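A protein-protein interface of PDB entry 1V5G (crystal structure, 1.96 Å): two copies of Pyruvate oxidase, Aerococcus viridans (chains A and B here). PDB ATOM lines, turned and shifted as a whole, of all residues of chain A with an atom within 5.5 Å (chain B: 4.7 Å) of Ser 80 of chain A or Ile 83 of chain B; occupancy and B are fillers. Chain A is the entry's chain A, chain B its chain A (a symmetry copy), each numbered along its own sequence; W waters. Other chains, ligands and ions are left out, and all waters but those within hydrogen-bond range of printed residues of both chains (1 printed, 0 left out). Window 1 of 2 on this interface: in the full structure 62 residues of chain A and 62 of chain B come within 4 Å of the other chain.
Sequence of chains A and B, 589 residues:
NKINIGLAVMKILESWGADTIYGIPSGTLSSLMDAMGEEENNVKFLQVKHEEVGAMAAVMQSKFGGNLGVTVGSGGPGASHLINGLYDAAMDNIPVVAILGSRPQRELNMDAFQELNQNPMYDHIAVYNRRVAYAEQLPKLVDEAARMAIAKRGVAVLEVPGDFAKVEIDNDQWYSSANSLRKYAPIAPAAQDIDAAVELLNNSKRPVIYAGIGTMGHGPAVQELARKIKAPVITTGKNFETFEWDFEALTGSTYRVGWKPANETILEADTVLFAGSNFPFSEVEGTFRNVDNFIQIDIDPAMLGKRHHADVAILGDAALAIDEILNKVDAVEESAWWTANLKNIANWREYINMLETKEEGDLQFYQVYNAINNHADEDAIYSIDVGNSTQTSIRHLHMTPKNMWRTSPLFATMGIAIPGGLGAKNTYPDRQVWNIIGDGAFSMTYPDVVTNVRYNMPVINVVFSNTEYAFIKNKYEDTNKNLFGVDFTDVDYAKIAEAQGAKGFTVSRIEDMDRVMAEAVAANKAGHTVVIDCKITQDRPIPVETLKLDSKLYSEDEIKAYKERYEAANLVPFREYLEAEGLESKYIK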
ATOM      1  N   SER A  74       7.831  27.473 -37.073  1.00  0.00           N
ATOM      2  CA  SER A  74       8.994  26.940 -37.774  1.00  0.00           C
ATOM      3  C   SER A  74       9.826  26.056 -36.846  1.00  0.00           C
ATOM      4  O   SER A  74       9.894  26.299 -35.642  1.00  0.00           O
ATOM      5  CB  SER A  74       9.858  28.082 -38.316  1.00  0.00           C
ATOM      6  OG  SER A  74      10.344  28.902 -37.272  1.00  0.00           O
ATOM      7  N   GLY A  76      12.037  24.334 -34.354  1.00  0.00           N
ATOM      8  CA  GLY A  76      12.844  24.910 -33.302  1.00  0.00           C
ATOM      9  C   GLY A  76      12.210  26.103 -32.607  1.00  0.00           C
ATOM     10  O   GLY A  76      11.228  25.947 -31.880  1.00  0.00           O
ATOM     11  N   PRO A  77      12.750  27.317 -32.816  1.00  0.00           N
ATOM     12  CA  PRO A  77      12.253  28.554 -32.206  1.00  0.00           C
ATOM     13  C   PRO A  77      10.830  28.991 -32.563  1.00  0.00           C
ATOM     14  O   PRO A  77      10.154  29.619 -31.755  1.00  0.00           O
ATOM     15  CB  PRO A  77      13.310  29.581 -32.610  1.00  0.00           C
ATOM     16  CG  PRO A  77      13.790  29.058 -33.941  1.00  0.00           C
ATOM     17  CD  PRO A  77      13.935  27.586 -33.652  1.00  0.00           C
ATOM     18  N   GLY A  78      10.379  28.674 -33.771  1.00  0.00           N
ATOM     19  CA  GLY A  78       9.033  29.057 -34.159  1.00  0.00           C
ATOM     20  C   GLY A  78       8.044  28.177 -33.423  1.00  0.00           C
ATOM     21  O   GLY A  78       7.043  28.652 -32.883  1.00  0.00           O
ATOM     22  N   ALA A  79       8.346  26.882 -33.400  1.00  0.00           N
ATOM     23  CA  ALA A  79       7.511  25.893 -32.736  1.00  0.00           C
ATOM     24  C   ALA A  79       7.463  26.130 -31.232  1.00  0.00           C
ATOM     25  O   ALA A  79       6.395  26.051 -30.628  1.00  0.00           O
ATOM     26  CB  ALA A  79       8.037  24.487 -33.030  1.00  0.00           C
ATOM     27  N   SER A  80       8.608  26.431 -30.622  1.00  0.00           N
ATOM     28  CA  SER A  80       8.628  26.654 -29.173  1.00  0.00           C
ATOM     29  C   SER A  80       7.846  27.902 -28.774  1.00  0.00           C
ATOM     30  O   SER A  80       7.320  27.983 -27.663  1.00  0.00           O
ATOM     31  CB  SER A  80      10.066  26.737 -28.652  1.00  0.00           C
ATOM     32  OG  SER A  80      10.822  27.723 -29.333  1.00  0.00           O
ATOM     33  N   HIS A  81       7.769  28.868 -29.687  1.00  0.00           N
ATOM     34  CA  HIS A  81       7.036  30.108 -29.450  1.00  0.00           C
ATOM     35  C   HIS A  81       5.529  29.875 -29.350  1.00  0.00           C
ATOM     36  O   HIS A  81       4.791  30.748 -28.910  1.00  0.00           O
ATOM     37  CB  HIS A  81       7.314  31.112 -30.575  1.00  0.00           C
ATOM     38  CG  HIS A  81       8.354  32.135 -30.235  1.00  0.00           C
ATOM     39  ND1 HIS A  81       8.807  33.066 -31.146  1.00  0.00           N
ATOM     40  CD2 HIS A  81       9.013  32.388 -29.079  1.00  0.00           C
ATOM     41  CE1 HIS A  81       9.701  33.848 -30.566  1.00  0.00           C
ATOM     42  NE2 HIS A  81       9.844  33.459 -29.312  1.00  0.00           N
ATOM     43  N   LEU A  82       5.074  28.693 -29.750  1.00  0.00           N
ATOM     44  CA  LEU A  82       3.652  28.381 -29.706  1.00  0.00           C
ATOM     45  C   LEU A  82       3.183  27.993 -28.311  1.00  0.00           C
ATOM     46  O   LEU A  82       1.991  28.040 -28.011  1.00  0.00           O
ATOM     47  CB  LEU A  82       3.336  27.212 -30.644  1.00  0.00           C
ATOM     48  CG  LEU A  82       3.788  27.295 -32.098  1.00  0.00           C
ATOM     49  CD1 LEU A  82       3.426  25.999 -32.807  1.00  0.00           C
ATOM     50  CD2 LEU A  82       3.151  28.491 -32.776  1.00  0.00           C
ATOM     51  N   ILE A  83       4.133  27.633 -27.460  1.00  0.00           N
ATOM     52  CA  ILE A  83       3.833  27.142 -26.123  1.00  0.00           C
ATOM     53  C   ILE A  83       2.744  27.805 -25.274  1.00  0.00           C
ATOM     54  O   ILE A  83       1.822  27.119 -24.825  1.00  0.00           O
ATOM     55  CB  ILE A  83       5.146  27.002 -25.296  1.00  0.00           C
ATOM     56  CG1 ILE A  83       4.881  26.139 -24.059  1.00  0.00           C
ATOM     57  CG2 ILE A  83       5.694  28.380 -24.921  1.00  0.00           C
ATOM     58  CD1 ILE A  83       6.142  25.601 -23.414  1.00  0.00           C
ATOM     59  N   ASN A  84       2.808  29.111 -25.045  1.00  0.00           N
ATOM     60  CA  ASN A  84       1.770  29.727 -24.214  1.00  0.00           C
ATOM     61  C   ASN A  84       0.364  29.571 -24.774  1.00  0.00           C
ATOM     62  O   ASN A  84      -0.601  29.450 -24.019  1.00  0.00           O
ATOM     63  CB  ASN A  84       2.076  31.204 -23.967  1.00  0.00           C
ATOM     64  CG  ASN A  84       3.109  31.390 -22.880  1.00  0.00           C
ATOM     65  OD1 ASN A  84       4.187  30.801 -22.936  1.00  0.00           O
ATOM     66  ND2 ASN A  84       2.784  32.195 -21.884  1.00  0.00           N
ATOM     67  N   MET A 121       8.751  18.309 -26.935  1.00  0.00           N
ATOM     68  CA  MET A 121       8.224  19.656 -26.729  1.00  0.00           C
ATOM     69  C   MET A 121       6.798  19.769 -26.197  1.00  0.00           C
ATOM     70  O   MET A 121       6.565  20.446 -25.191  1.00  0.00           O
ATOM     71  CB  MET A 121       8.353  20.475 -28.021  1.00  0.00           C
ATOM     72  CG  MET A 121       8.249  21.984 -27.798  1.00  0.00           C
ATOM     73  SD  MET A 121       8.552  22.942 -29.296  1.00  0.00           S
ATOM     74  CE  MET A 121      10.340  22.734 -29.469  1.00  0.00           C
ATOM     75  N   TYR A 122       5.846  19.110 -26.853  1.00  0.00           N
ATOM     76  CA  TYR A 122       4.452  19.200 -26.418  1.00  0.00           C
ATOM     77  C   TYR A 122       3.763  17.871 -26.110  1.00  0.00           C
ATOM     78  O   TYR A 122       2.533  17.802 -26.045  1.00  0.00           O
ATOM     79  CB  TYR A 122       3.645  19.965 -27.469  1.00  0.00           C
ATOM     80  CG  TYR A 122       4.134  21.387 -27.685  1.00  0.00           C
ATOM     81  CD1 TYR A 122       4.142  22.305 -26.634  1.00  0.00           C
ATOM     82  CD2 TYR A 122       4.589  21.813 -28.935  1.00  0.00           C
ATOM     83  CE1 TYR A 122       4.588  23.611 -26.819  1.00  0.00           C
ATOM     84  CE2 TYR A 122       5.040  23.123 -29.130  1.00  0.00           C
ATOM     85  CZ  TYR A 122       5.032  24.014 -28.064  1.00  0.00           C
ATOM     86  OH  TYR A 122       5.446  25.313 -28.247  1.00  0.00           O
ATOM     87  N   ALA B  79       6.911  30.751 -16.778  1.00  0.00           N
ATOM     88  CA  ALA B  79       7.892  29.692 -16.953  1.00  0.00           C
ATOM     89  C   ALA B  79       7.957  29.231 -18.403  1.00  0.00           C
ATOM     90  O   ALA B  79       9.045  29.034 -18.941  1.00  0.00           O
ATOM     91  CB  ALA B  79       7.553  28.512 -16.041  1.00  0.00           C
ATOM     92  N   SER B  80       6.802  29.067 -19.047  1.00  0.00           N
ATOM     93  CA  SER B  80       6.799  28.609 -20.439  1.00  0.00           C
ATOM     94  C   SER B  80       7.418  29.638 -21.382  1.00  0.00           C
ATOM     95  O   SER B  80       7.963  29.280 -22.427  1.00  0.00           O
ATOM     96  CB  SER B  80       5.380  28.253 -20.895  1.00  0.00           C
ATOM     97  OG  SER B  80       4.476  29.328 -20.706  1.00  0.00           O
ATOM     98  N   HIS B  81       7.333  30.911 -21.004  1.00  0.00           N
ATOM     99  CA  HIS B  81       7.899  31.998 -21.797  1.00  0.00           C
ATOM    100  C   HIS B  81       9.426  31.952 -21.830  1.00  0.00           C
ATOM    101  O   HIS B  81      10.053  32.625 -22.639  1.00  0.00           O
ATOM    102  CB  HIS B  81       7.451  33.353 -21.235  1.00  0.00           C
ATOM    103  CG  HIS B  81       6.294  33.962 -21.966  1.00  0.00           C
ATOM    104  ND1 HIS B  81       5.690  35.133 -21.557  1.00  0.00           N
ATOM    105  CD2 HIS B  81       5.644  33.577 -23.090  1.00  0.00           C
ATOM    106  CE1 HIS B  81       4.717  35.441 -22.398  1.00  0.00           C
ATOM    107  NE2 HIS B  81       4.669  34.515 -23.337  1.00  0.00           N
ATOM    108  N   LEU B  82      10.023  31.150 -20.956  1.00  0.00           N
ATOM    109  CA  LEU B  82      11.475  31.047 -20.901  1.00  0.00           C
ATOM    110  C   LEU B  82      12.038  30.141 -21.986  1.00  0.00           C
ATOM    111  O   LEU B  82      13.221  30.209 -22.314  1.00  0.00           O
ATOM    112  CB  LEU B  82      11.916  30.481 -19.549  1.00  0.00           C
ATOM    113  CG  LEU B  82      11.410  31.147 -18.274  1.00  0.00           C
ATOM    114  CD1 LEU B  82      11.921  30.370 -17.069  1.00  0.00           C
ATOM    115  CD2 LEU B  82      11.857  32.594 -18.227  1.00  0.00           C
ATOM    116  N   ILE B  83      11.173  29.311 -22.553  1.00  0.00           N
ATOM    117  CA  ILE B  83      11.580  28.317 -23.536  1.00  0.00           C
ATOM    118  C   ILE B  83      12.596  28.668 -24.627  1.00  0.00           C
ATOM    119  O   ILE B  83      13.617  27.985 -24.749  1.00  0.00           O
ATOM    120  CB  ILE B  83      10.325  27.644 -24.169  1.00  0.00           C
ATOM    121  CG1 ILE B  83      10.745  26.361 -24.892  1.00  0.00           C
ATOM    122  CG2 ILE B  83       9.608  28.618 -25.105  1.00  0.00           C
ATOM    123  CD1 ILE B  83       9.589  25.426 -25.186  1.00  0.00           C
ATOM    124  N   ASN B  84      12.364  29.709 -25.417  1.00  0.00           N
ATOM    125  CA  ASN B  84      13.335  30.020 -26.469  1.00  0.00           C
ATOM    126  C   ASN B  84      14.730  30.324 -25.945  1.00  0.00           C
ATOM    127  O   ASN B  84      15.726  30.009 -26.596  1.00  0.00           O
ATOM    128  CB  ASN B  84      12.839  31.171 -27.344  1.00  0.00           C
ATOM    129  CG  ASN B  84      11.827  30.706 -28.364  1.00  0.00           C
ATOM    130  OD1 ASN B  84      10.837  30.066 -28.015  1.00  0.00           O
ATOM    131  ND2 ASN B  84      12.071  31.013 -29.626  1.00  0.00           N
ATOM    132  N   GLY B  85      14.798  30.933 -24.767  1.00  0.00           N
ATOM    133  CA  GLY B  85      16.084  31.246 -24.178  1.00  0.00           C
ATOM    134  C   GLY B  85      16.768  30.013 -23.619  1.00  0.00           C
ATOM    135  O   GLY B  85      17.990  29.883 -23.701  1.00  0.00           O
ATOM    136  N   LEU B  86      15.983  29.096 -23.056  1.00  0.00           N
ATOM    137  CA  LEU B  86      16.541  27.881 -22.479  1.00  0.00           C
ATOM    138  C   LEU B  86      16.994  26.892 -23.551  1.00  0.00           C
ATOM    139  O   LEU B  86      18.010  26.220 -23.384  1.00  0.00           O
ATOM    140  CB  LEU B  86      15.517  27.220 -21.550  1.00  0.00           C
ATOM    141  CG  LEU B  86      15.045  28.120 -20.406  1.00  0.00           C
ATOM    142  CD1 LEU B  86      14.138  27.330 -19.459  1.00  0.00           C
ATOM    143  CD2 LEU B  86      16.260  28.658 -19.667  1.00  0.00           C
ATOM    144  N   TYR B  87      16.241  26.800 -24.643  1.00  0.00           N
ATOM    145  CA  TYR B  87      16.600  25.900 -25.733  1.00  0.00           C
ATOM    146  C   TYR B  87      17.880  26.388 -26.393  1.00  0.00           C
ATOM    147  O   TYR B  87      18.706  25.588 -26.836  1.00  0.00           O
ATOM    148  CB  TYR B  87      15.472  25.824 -26.764  1.00  0.00           C
ATOM    149  CG  TYR B  87      14.571  24.620 -26.597  1.00  0.00           C
ATOM    150  CD1 TYR B  87      14.678  23.515 -27.450  1.00  0.00           C
ATOM    151  CD2 TYR B  87      13.619  24.577 -25.581  1.00  0.00           C
ATOM    152  CE1 TYR B  87      13.849  22.398 -27.292  1.00  0.00           C
ATOM    153  CE2 TYR B  87      12.790  23.470 -25.412  1.00  0.00           C
ATOM    154  CZ  TYR B  87      12.909  22.387 -26.268  1.00  0.00           C
ATOM    155  OH  TYR B  87      12.080  21.303 -26.095  1.00  0.00           O
ATOM    156  N   TYR B 122      10.651  21.283 -19.206  1.00  0.00           N
ATOM    157  CA  TYR B 122      12.033  21.355 -19.679  1.00  0.00           C
ATOM    158  C   TYR B 122      12.905  20.137 -19.380  1.00  0.00           C
ATOM    159  O   TYR B 122      14.134  20.213 -19.446  1.00  0.00           O
ATOM    160  CB  TYR B 122      12.694  22.613 -19.112  1.00  0.00           C
ATOM    161  CG  TYR B 122      12.011  23.899 -19.543  1.00  0.00           C
ATOM    162  CD1 TYR B 122      11.912  24.236 -20.893  1.00  0.00           C
ATOM    163  CD2 TYR B 122      11.462  24.776 -18.604  1.00  0.00           C
ATOM    164  CE1 TYR B 122      11.288  25.411 -21.302  1.00  0.00           C
ATOM    165  CE2 TYR B 122      10.831  25.958 -19.005  1.00  0.00           C
ATOM    166  CZ  TYR B 122      10.753  26.266 -20.357  1.00  0.00           C
ATOM    167  OH  TYR B 122      10.161  27.440 -20.765  1.00  0.00           O
ATOM    168  N   PHE B 411      20.263  26.887 -32.374  1.00  0.00           N
ATOM    169  CA  PHE B 411      18.812  26.826 -32.209  1.00  0.00           C
ATOM    170  C   PHE B 411      18.286  27.937 -33.118  1.00  0.00           C
ATOM    171  O   PHE B 411      17.203  27.837 -33.696  1.00  0.00           O
ATOM    172  CB  PHE B 411      18.426  27.092 -30.749  1.00  0.00           C
ATOM    173  CG  PHE B 411      16.943  26.965 -30.469  1.00  0.00           C
ATOM    174  CD1 PHE B 411      16.273  25.760 -30.689  1.00  0.00           C
ATOM    175  CD2 PHE B 411      16.227  28.041 -29.940  1.00  0.00           C
ATOM    176  CE1 PHE B 411      14.920  25.629 -30.385  1.00  0.00           C
ATOM    177  CE2 PHE B 411      14.869  27.919 -29.632  1.00  0.00           C
ATOM    178  CZ  PHE B 411      14.216  26.711 -29.853  1.00  0.00           C
HETATM  179  O   HOH W   1      11.335  19.024 -28.009  1.00  0.00           O
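The backbone carbonyl oxygen (O) of Gly 76 of chain A lies within hydrogen-bond range of the side-chain hydroxyl (OG) of Ser 80 of chain A, at 3.1 Å.
The backbone NH (N) of Ser 80 of chain A sits close to the side-chain sulfur (SD) of Met 121 of chain A, 3.7 Å away.
The side-chain hydroxyl (OH) of Tyr 122 of chain A lies within hydrogen-bond range of the backbone carbonyl oxygen (O) of Ser 80 of chain A.
The backbone carbonyl oxygen (O) of Pro 77 of chain A sits at hydrogen-bond distance from the side-chain hydroxyl (OG) of Ser 80 of chain A (3.1 Å).
O of Ser 80 of chain B is in hydrogen-bond range of OH of Tyr 122 of chain B (3.3 Å).
The backbone NH of Ile 83 of chain B lies within hydrogen-bond range of the side-chain hydroxyl of Tyr 122 of chain B (2.8 Å).
Ser 80 of chain A touches Ile 83 of chain B, and with the chains exchanged Ile 83 of chain A touches Ser 80 of chain B.
Ser 80 of chain A touches Asn 84 of chain B, and with the chains exchanged Asn 84 of chain A touches Ser 80 of chain B.
His 81 of chain A touches Asn 84 of chain B, and with the chains exchanged Asn 84 of chain A touches His 81 of chain B.
Ile 83 of chain A touches its own counterpart, Ile 83 of chain B.
OD1 of Asn 84 of chain B sits at hydrogen-bond distance from OG of Ser 80 of chain A.
A ring nitrogen (NE2) of His 81 of chain A is in hydrogen-bond range of the side-chain amide nitrogen of Asn 84 of chain B, at 3.3 Å.
O of Pro 77 of chain A lies within hydrogen-bond range of ND2 of Asn 84 of chain B (3.2 Å).
OG of Ser 80 of chain B lies within hydrogen-bond range of OD1 of Asn 84 of chain A, at 2.7 Å.
The side-chain amide nitrogen of Asn 84 of chain A is in hydrogen-bond range of a ring nitrogen (NE2) of His 81 of chain B, at 3.3 Å.
Among the printed residues, merely in contact across the chains: Gly 76 of chain A with Phe 411 of chain B (3.5 Å), Pro 77 of chain A with Phe 411 of chain B (3.3 Å), Ser 80 of chain A with Ile 83 of chain B (3.5 Å), Ser 80 of chain A with Phe 411 of chain B (3.6 Å), Ile 83 of chain A with Ser 80 of chain B (3.5 Å) and Ile 83 of chain A with Ile 83 of chain B (3.9 Å).
Water W1 lies within hydrogen-bond range of the backbone NH (N) of Met 121 of chain A (2.9 Å) and the side-chain hydroxyl (OH) of Tyr 87 of chain B (3.1 Å).
Ser 80 of chain A touches three residues of chain B.
Ile 83 of chain B touches just these residues of chain A: Ser 80 (3.5 Å) and Ile 83 (3.9 Å).
Of the printed residues of chain B, His 81 of chain A touches Asn 84 (3.1 Å).
Printed residues of chain B within 4 Å of Ile 83 of chain A: Ser 80 (3.5 Å) and Ile 83 (3.9 Å).
Printed residues of chain A within 4 Å of His 81 of chain B: Asn 84 (3.1 Å).
Of the printed residues of chain B, Gly 76 of chain A touches Phe 411.
Printed residues of chain A within 4 Å of Asn 84 of chain B: Pro 77 (3.2 Å), Ser 80 (2.7 Å) and His 81 (3.1 Å).
The nearest residue of chain A that does not touch Ile 83 of chain B is Met 121 of chain A (4.5 Å).
Of the 12 printed residues of chain A, 6 touch a printed residue of chain B.
Hydrophobic or aromatic side chains of chain A within 4 Å of the printed part of chain B: Pro 77, His 81 and Ile 83.
Printed residues of chain B that touch a printed residue of chain A: Ser 80, His 81, Ile 83, Asn 84 and Phe 411.
Hydrophobic or aromatic side chains of chain B that line the printed part of chain A: His 81, Ile 83 and Phe 411.
Among the printed residues, 11 pairs touch across the chains.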
